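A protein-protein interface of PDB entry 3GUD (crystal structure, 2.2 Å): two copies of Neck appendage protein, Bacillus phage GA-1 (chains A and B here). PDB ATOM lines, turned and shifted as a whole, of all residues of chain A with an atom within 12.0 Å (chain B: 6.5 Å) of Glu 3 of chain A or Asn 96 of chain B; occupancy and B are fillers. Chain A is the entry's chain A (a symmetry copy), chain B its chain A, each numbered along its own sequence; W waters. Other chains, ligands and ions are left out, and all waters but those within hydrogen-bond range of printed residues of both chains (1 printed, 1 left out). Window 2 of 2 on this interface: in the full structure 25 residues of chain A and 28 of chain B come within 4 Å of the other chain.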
ATOM      1  N   GLU A   3      16.356   5.539  -5.789  1.00  0.00           N
ATOM      2  CA  GLU A   3      16.192   4.259  -6.473  1.00  0.00           C
ATOM      3  C   GLU A   3      14.990   4.291  -7.389  1.00  0.00           C
ATOM      4  O   GLU A   3      14.362   5.343  -7.582  1.00  0.00           O
ATOM      5  CB  GLU A   3      16.005   3.095  -5.479  1.00  0.00           C
ATOM      6  CG  GLU A   3      17.297   2.413  -4.983  1.00  0.00           C
ATOM      7  CD  GLU A   3      17.980   3.194  -3.892  1.00  0.00           C
ATOM      8  OE1 GLU A   3      18.625   2.580  -3.021  1.00  0.00           O
ATOM      9  OE2 GLU A   3      17.844   4.430  -3.909  1.00  0.00           O
ATOM     10  N   ARG A   4      14.667   3.113  -7.936  1.00  0.00           N
ATOM     11  CA  ARG A   4      13.393   2.919  -8.628  1.00  0.00           C
ATOM     12  C   ARG A   4      12.285   2.249  -7.794  1.00  0.00           C
ATOM     13  O   ARG A   4      12.359   1.068  -7.391  1.00  0.00           O
ATOM     14  CB  ARG A   4      13.532   2.447 -10.087  1.00  0.00           C
ATOM     15  CG  ARG A   4      13.429   3.709 -10.951  1.00  0.00           C
ATOM     16  CD  ARG A   4      13.630   4.929  -9.999  1.00  0.00           C
ATOM     17  NE  ARG A   4      13.378   6.268 -10.554  1.00  0.00           N
ATOM     18  CZ  ARG A   4      13.314   7.376  -9.809  1.00  0.00           C
ATOM     19  NH1 ARG A   4      13.076   8.584 -10.354  1.00  0.00           N
ATOM     20  NH2 ARG A   4      13.445   7.252  -8.493  1.00  0.00           N
ATOM     21  N   HIS A   5      11.306   3.100  -7.474  1.00  0.00           N
ATOM     22  CA  HIS A   5      10.029   2.729  -6.887  1.00  0.00           C
ATOM     23  C   HIS A   5       9.048   2.479  -8.042  1.00  0.00           C
ATOM     24  O   HIS A   5       7.828   2.535  -7.865  1.00  0.00           O
ATOM     25  CB  HIS A   5       9.540   3.866  -5.974  1.00  0.00           C
ATOM     26  CG  HIS A   5      10.488   4.173  -4.856  1.00  0.00           C
ATOM     27  ND1 HIS A   5      10.127   4.899  -3.733  1.00  0.00           N
ATOM     28  CD2 HIS A   5      11.782   3.833  -4.671  1.00  0.00           C
ATOM     29  CE1 HIS A   5      11.162   5.001  -2.924  1.00  0.00           C
ATOM     30  NE2 HIS A   5      12.187   4.356  -3.471  1.00  0.00           N
ATOM     31  N   LYS A   6       9.620   2.169  -9.212  1.00  0.00           N
ATOM     32  CA  LYS A   6       8.887   2.042 -10.471  1.00  0.00           C
ATOM     33  C   LYS A   6       8.844   0.612 -11.046  1.00  0.00           C
ATOM     34  O   LYS A   6       9.606  -0.259 -10.638  1.00  0.00           O
ATOM     35  CB  LYS A   6       9.436   3.034 -11.500  1.00  0.00           C
ATOM     36  CG  LYS A   6       9.027   4.452 -11.183  1.00  0.00           C
ATOM     37  CD  LYS A   6       9.762   5.483 -12.009  1.00  0.00           C
ATOM     38  CE  LYS A   6       9.620   6.874 -11.376  1.00  0.00           C
ATOM     39  NZ  LYS A   6      10.492   7.920 -11.999  1.00  0.00           N
ATOM     40  N   THR A   7       7.927   0.373 -11.981  1.00  0.00           N
ATOM     41  CA  THR A   7       7.751  -0.943 -12.595  1.00  0.00           C
ATOM     42  C   THR A   7       7.086  -0.764 -13.948  1.00  0.00           C
ATOM     43  O   THR A   7       6.956   0.363 -14.431  1.00  0.00           O
ATOM     44  CB  THR A   7       6.877  -1.868 -11.723  1.00  0.00           C
ATOM     45  OG1 THR A   7       6.765  -3.156 -12.338  1.00  0.00           O
ATOM     46  CG2 THR A   7       5.482  -1.287 -11.544  1.00  0.00           C
ATOM     47  N   ILE A   9       8.082  -0.863 -16.585  1.00  0.00           N
ATOM     48  CA  ILE A   9       8.954   0.166 -17.107  1.00  0.00           C
ATOM     49  C   ILE A   9       9.321  -0.158 -18.552  1.00  0.00           C
ATOM     50  O   ILE A   9       9.658  -1.299 -18.887  1.00  0.00           O
ATOM     51  CB  ILE A   9      10.206   0.270 -16.234  1.00  0.00           C
ATOM     52  CG1 ILE A   9      10.803   1.671 -16.312  1.00  0.00           C
ATOM     53  CG2 ILE A   9      11.198  -0.791 -16.635  1.00  0.00           C
ATOM     54  CD1 ILE A   9      11.296   2.035 -17.697  1.00  0.00           C
ATOM     55  N   GLN B  50      18.377   7.774 -12.374  1.00  0.00           N
ATOM     56  CA  GLN B  50      19.571   6.943 -12.429  1.00  0.00           C
ATOM     57  C   GLN B  50      20.147   6.876 -13.809  1.00  0.00           C
ATOM     58  O   GLN B  50      21.350   6.875 -13.975  1.00  0.00           O
ATOM     59  CB  GLN B  50      19.286   5.519 -11.969  1.00  0.00           C
ATOM     60  CG  GLN B  50      19.283   5.344 -10.470  1.00  0.00           C
ATOM     61  CD  GLN B  50      17.959   5.717  -9.853  1.00  0.00           C
ATOM     62  OE1 GLN B  50      17.140   6.389 -10.481  1.00  0.00           O
ATOM     63  NE2 GLN B  50      17.735   5.279  -8.613  1.00  0.00           N
ATOM     64  N   TYR B  71      19.361  13.783  -4.741  1.00  0.00           N
ATOM     65  CA  TYR B  71      19.614  12.555  -3.986  1.00  0.00           C
ATOM     66  C   TYR B  71      19.232  12.790  -2.543  1.00  0.00           C
ATOM     67  O   TYR B  71      19.422  13.866  -2.006  1.00  0.00           O
ATOM     68  CB  TYR B  71      21.070  12.089  -4.083  1.00  0.00           C
ATOM     69  CG  TYR B  71      21.367  10.859  -3.238  1.00  0.00           C
ATOM     70  CD1 TYR B  71      21.139   9.573  -3.730  1.00  0.00           C
ATOM     71  CD2 TYR B  71      21.884  10.988  -1.954  1.00  0.00           C
ATOM     72  CE1 TYR B  71      21.423   8.450  -2.963  1.00  0.00           C
ATOM     73  CE2 TYR B  71      22.176   9.882  -1.183  1.00  0.00           C
ATOM     74  CZ  TYR B  71      21.945   8.620  -1.685  1.00  0.00           C
ATOM     75  OH  TYR B  71      22.244   7.546  -0.887  1.00  0.00           O
ATOM     76  N   ASP B  72      18.673  11.753  -1.954  1.00  0.00           N
ATOM     77  CA  ASP B  72      18.133  11.858  -0.618  1.00  0.00           C
ATOM     78  C   ASP B  72      18.364  10.557   0.110  1.00  0.00           C
ATOM     79  O   ASP B  72      18.264   9.447  -0.440  1.00  0.00           O
ATOM     80  CB  ASP B  72      16.638  12.248  -0.603  1.00  0.00           C
ATOM     81  CG  ASP B  72      16.115  12.541   0.816  1.00  0.00           C
ATOM     82  OD1 ASP B  72      16.947  12.718   1.730  1.00  0.00           O
ATOM     83  OD2 ASP B  72      14.877  12.597   0.976  1.00  0.00           O
ATOM     84  N   GLU B  73      18.766  10.707   1.369  1.00  0.00           N
ATOM     85  CA  GLU B  73      19.146   9.558   2.183  1.00  0.00           C
ATOM     86  C   GLU B  73      18.706   9.717   3.633  1.00  0.00           C
ATOM     87  O   GLU B  73      18.601  10.846   4.139  1.00  0.00           O
ATOM     88  CB  GLU B  73      20.651   9.347   2.101  1.00  0.00           C
ATOM     89  CG  GLU B  73      21.295   8.921   3.413  1.00  0.00           C
ATOM     90  CD  GLU B  73      21.972  10.067   4.158  1.00  0.00           C
ATOM     91  OE1 GLU B  73      22.247  11.122   3.537  1.00  0.00           O
ATOM     92  OE2 GLU B  73      22.237   9.888   5.367  1.00  0.00           O
ATOM     93  N   TRP B  74      18.451   8.604   4.316  1.00  0.00           N
ATOM     94  CA  TRP B  74      17.845   8.708   5.651  1.00  0.00           C
ATOM     95  C   TRP B  74      18.242   7.676   6.717  1.00  0.00           C
ATOM     96  O   TRP B  74      18.767   6.599   6.417  1.00  0.00           O
ATOM     97  CB  TRP B  74      16.314   8.813   5.567  1.00  0.00           C
ATOM     98  CG  TRP B  74      15.625   7.698   4.863  1.00  0.00           C
ATOM     99  CD1 TRP B  74      15.241   6.494   5.387  1.00  0.00           C
ATOM    100  CD2 TRP B  74      15.191   7.703   3.498  1.00  0.00           C
ATOM    101  NE1 TRP B  74      14.605   5.746   4.420  1.00  0.00           N
ATOM    102  CE2 TRP B  74      14.566   6.467   3.250  1.00  0.00           C
ATOM    103  CE3 TRP B  74      15.279   8.637   2.457  1.00  0.00           C
ATOM    104  CZ2 TRP B  74      14.029   6.142   1.991  1.00  0.00           C
ATOM    105  CZ3 TRP B  74      14.753   8.316   1.212  1.00  0.00           C
ATOM    106  CH2 TRP B  74      14.135   7.084   0.991  1.00  0.00           C
ATOM    107  N   ALA B  94      16.129   2.224   6.847  1.00  0.00           N
ATOM    108  CA  ALA B  94      17.029   3.113   6.122  1.00  0.00           C
ATOM    109  C   ALA B  94      16.988   2.833   4.625  1.00  0.00           C
ATOM    110  O   ALA B  94      17.017   1.674   4.197  1.00  0.00           O
ATOM    111  CB  ALA B  94      18.451   2.975   6.650  1.00  0.00           C
ATOM    112  N   GLY B  95      16.918   3.903   3.836  1.00  0.00           N
ATOM    113  CA  GLY B  95      16.932   3.799   2.389  1.00  0.00           C
ATOM    114  C   GLY B  95      17.480   5.071   1.783  1.00  0.00           C
ATOM    115  O   GLY B  95      17.963   5.948   2.495  1.00  0.00           O
ATOM    116  N   ASN B  96      17.425   5.162   0.463  1.00  0.00           N
ATOM    117  CA  ASN B  96      17.744   6.398  -0.230  1.00  0.00           C
ATOM    118  C   ASN B  96      16.856   6.474  -1.449  1.00  0.00           C
ATOM    119  O   ASN B  96      16.078   5.555  -1.718  1.00  0.00           O
ATOM    120  CB  ASN B  96      19.225   6.467  -0.635  1.00  0.00           C
ATOM    121  CG  ASN B  96      19.685   5.239  -1.399  1.00  0.00           C
ATOM    122  OD1 ASN B  96      19.598   5.186  -2.624  1.00  0.00           O
ATOM    123  ND2 ASN B  96      20.169   4.238  -0.673  1.00  0.00           N
ATOM    124  N   ILE B  97      16.972   7.559  -2.198  1.00  0.00           N
ATOM    125  CA  ILE B  97      16.086   7.756  -3.321  1.00  0.00           C
ATOM    126  C   ILE B  97      16.634   8.870  -4.188  1.00  0.00           C
ATOM    127  O   ILE B  97      17.077   9.894  -3.680  1.00  0.00           O
ATOM    128  CB  ILE B  97      14.655   8.093  -2.820  1.00  0.00           C
ATOM    129  CG1 ILE B  97      13.634   8.035  -3.956  1.00  0.00           C
ATOM    130  CG2 ILE B  97      14.626   9.437  -2.128  1.00  0.00           C
ATOM    131  CD1 ILE B  97      12.325   8.723  -3.620  1.00  0.00           C
ATOM    132  N   TYR B  98      16.634   8.644  -5.497  1.00  0.00           N
ATOM    133  CA  TYR B  98      16.930   9.691  -6.460  1.00  0.00           C
ATOM    134  C   TYR B  98      15.622  10.175  -7.054  1.00  0.00           C
ATOM    135  O   TYR B  98      14.743   9.377  -7.373  1.00  0.00           O
ATOM    136  CB  TYR B  98      17.815   9.159  -7.578  1.00  0.00           C
ATOM    137  CG  TYR B  98      19.242   8.886  -7.168  1.00  0.00           C
ATOM    138  CD1 TYR B  98      19.583   7.710  -6.505  1.00  0.00           C
ATOM    139  CD2 TYR B  98      20.256   9.798  -7.461  1.00  0.00           C
ATOM    140  CE1 TYR B  98      20.899   7.447  -6.135  1.00  0.00           C
ATOM    141  CE2 TYR B  98      21.578   9.550  -7.096  1.00  0.00           C
ATOM    142  CZ  TYR B  98      21.896   8.368  -6.435  1.00  0.00           C
ATOM    143  OH  TYR B  98      23.202   8.107  -6.071  1.00  0.00           O
ATOM    144  N   SER B  99      15.485  11.484  -7.187  1.00  0.00           N
ATOM    145  CA  SER B  99      14.294  12.065  -7.777  1.00  0.00           C
ATOM    146  C   SER B  99      14.784  12.902  -8.926  1.00  0.00           C
ATOM    147  O   SER B  99      15.962  12.880  -9.222  1.00  0.00           O
ATOM    148  CB  SER B  99      13.544  12.933  -6.757  1.00  0.00           C
ATOM    149  OG  SER B  99      14.373  13.940  -6.203  1.00  0.00           O
HETATM  150  O   HOH W   1      11.870   8.697  -6.455  1.00  0.00           O
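No position is printed for both chains.
O of Asp 72 of chain B lies within hydrogen-bond range of N of Ile 97 of chain B, 2.9 Å away.
The backbone carbonyl oxygen of Tyr 98 of chain B is in hydrogen-bond range of the guanidinium group of Arg 4 of chain A, at 2.7 Å. The backbone NH (N) of Glu 3 of chain A lies close to the backbone NH (N) of Tyr 98 of chain B (3.1 Å). NE2 of Gln 50 of chain B sits close to N of Glu 3 of chain A, 3.2 Å away. The side-chain amide oxygen (OD1) of Asn 96 of chain B sits close to the side-chain carboxylate (OE1) of Glu 3 of chain A (2.8 Å).
Glu 3 of chain A touches just these residues of chain B: Gln 50 (2.8 Å), Asn 96 (2.3 Å), Ile 97 (3.3 Å) and Tyr 98 (3.1 Å). Of the printed residues of chain B, Arg 4 of chain A touches Gln 50 and Tyr 98. Printed residues of chain B within 4 Å of His 5 of chain A: Ile 97 (3.96 Å). Thr 7 of chain A touches none of the printed residues of chain B. Of the printed residues of chain A, Gln 50 of chain B touches Glu 3 (2.8 Å) and Arg 4 (3.8 Å). Tyr 71 of chain B touches none of the printed residues of chain A. Glu 73 of chain B touches none of the printed residues of chain A. No residue of chain A comes within 4 Å of Trp 74 of chain B. No residue of chain A comes within 4 Å of Gly 95 of chain B. Asn 96 of chain B touches just one residue of chain A: Glu 3 (2.3 Å). The nearest printed residue of chain B that does not touch His 5 of chain A is Asn 96 of chain B (4.4 Å).
Water W1 bridges NH2 of Arg 4 of chain A and O of Tyr 98 of chain B.
Hydrophobic or aromatic side chains of chain A within 4 Å of the printed part of chain B: His 5. Of the 11 printed residues of chain B, 4 touch a printed residue of chain A. Printed residues of chain B that touch a printed residue of chain A: Gln 50, Asn 96, Ile 97 and Tyr 98.
N of Glu 3 of chain A touches CA of Ile 97 of chain B (3.3 Å). OE1 of Gln 50 of chain B touches NE of Arg 4 of chain A, at 3.8 Å. His 5 of chain A touches Ile 97 of chain B.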
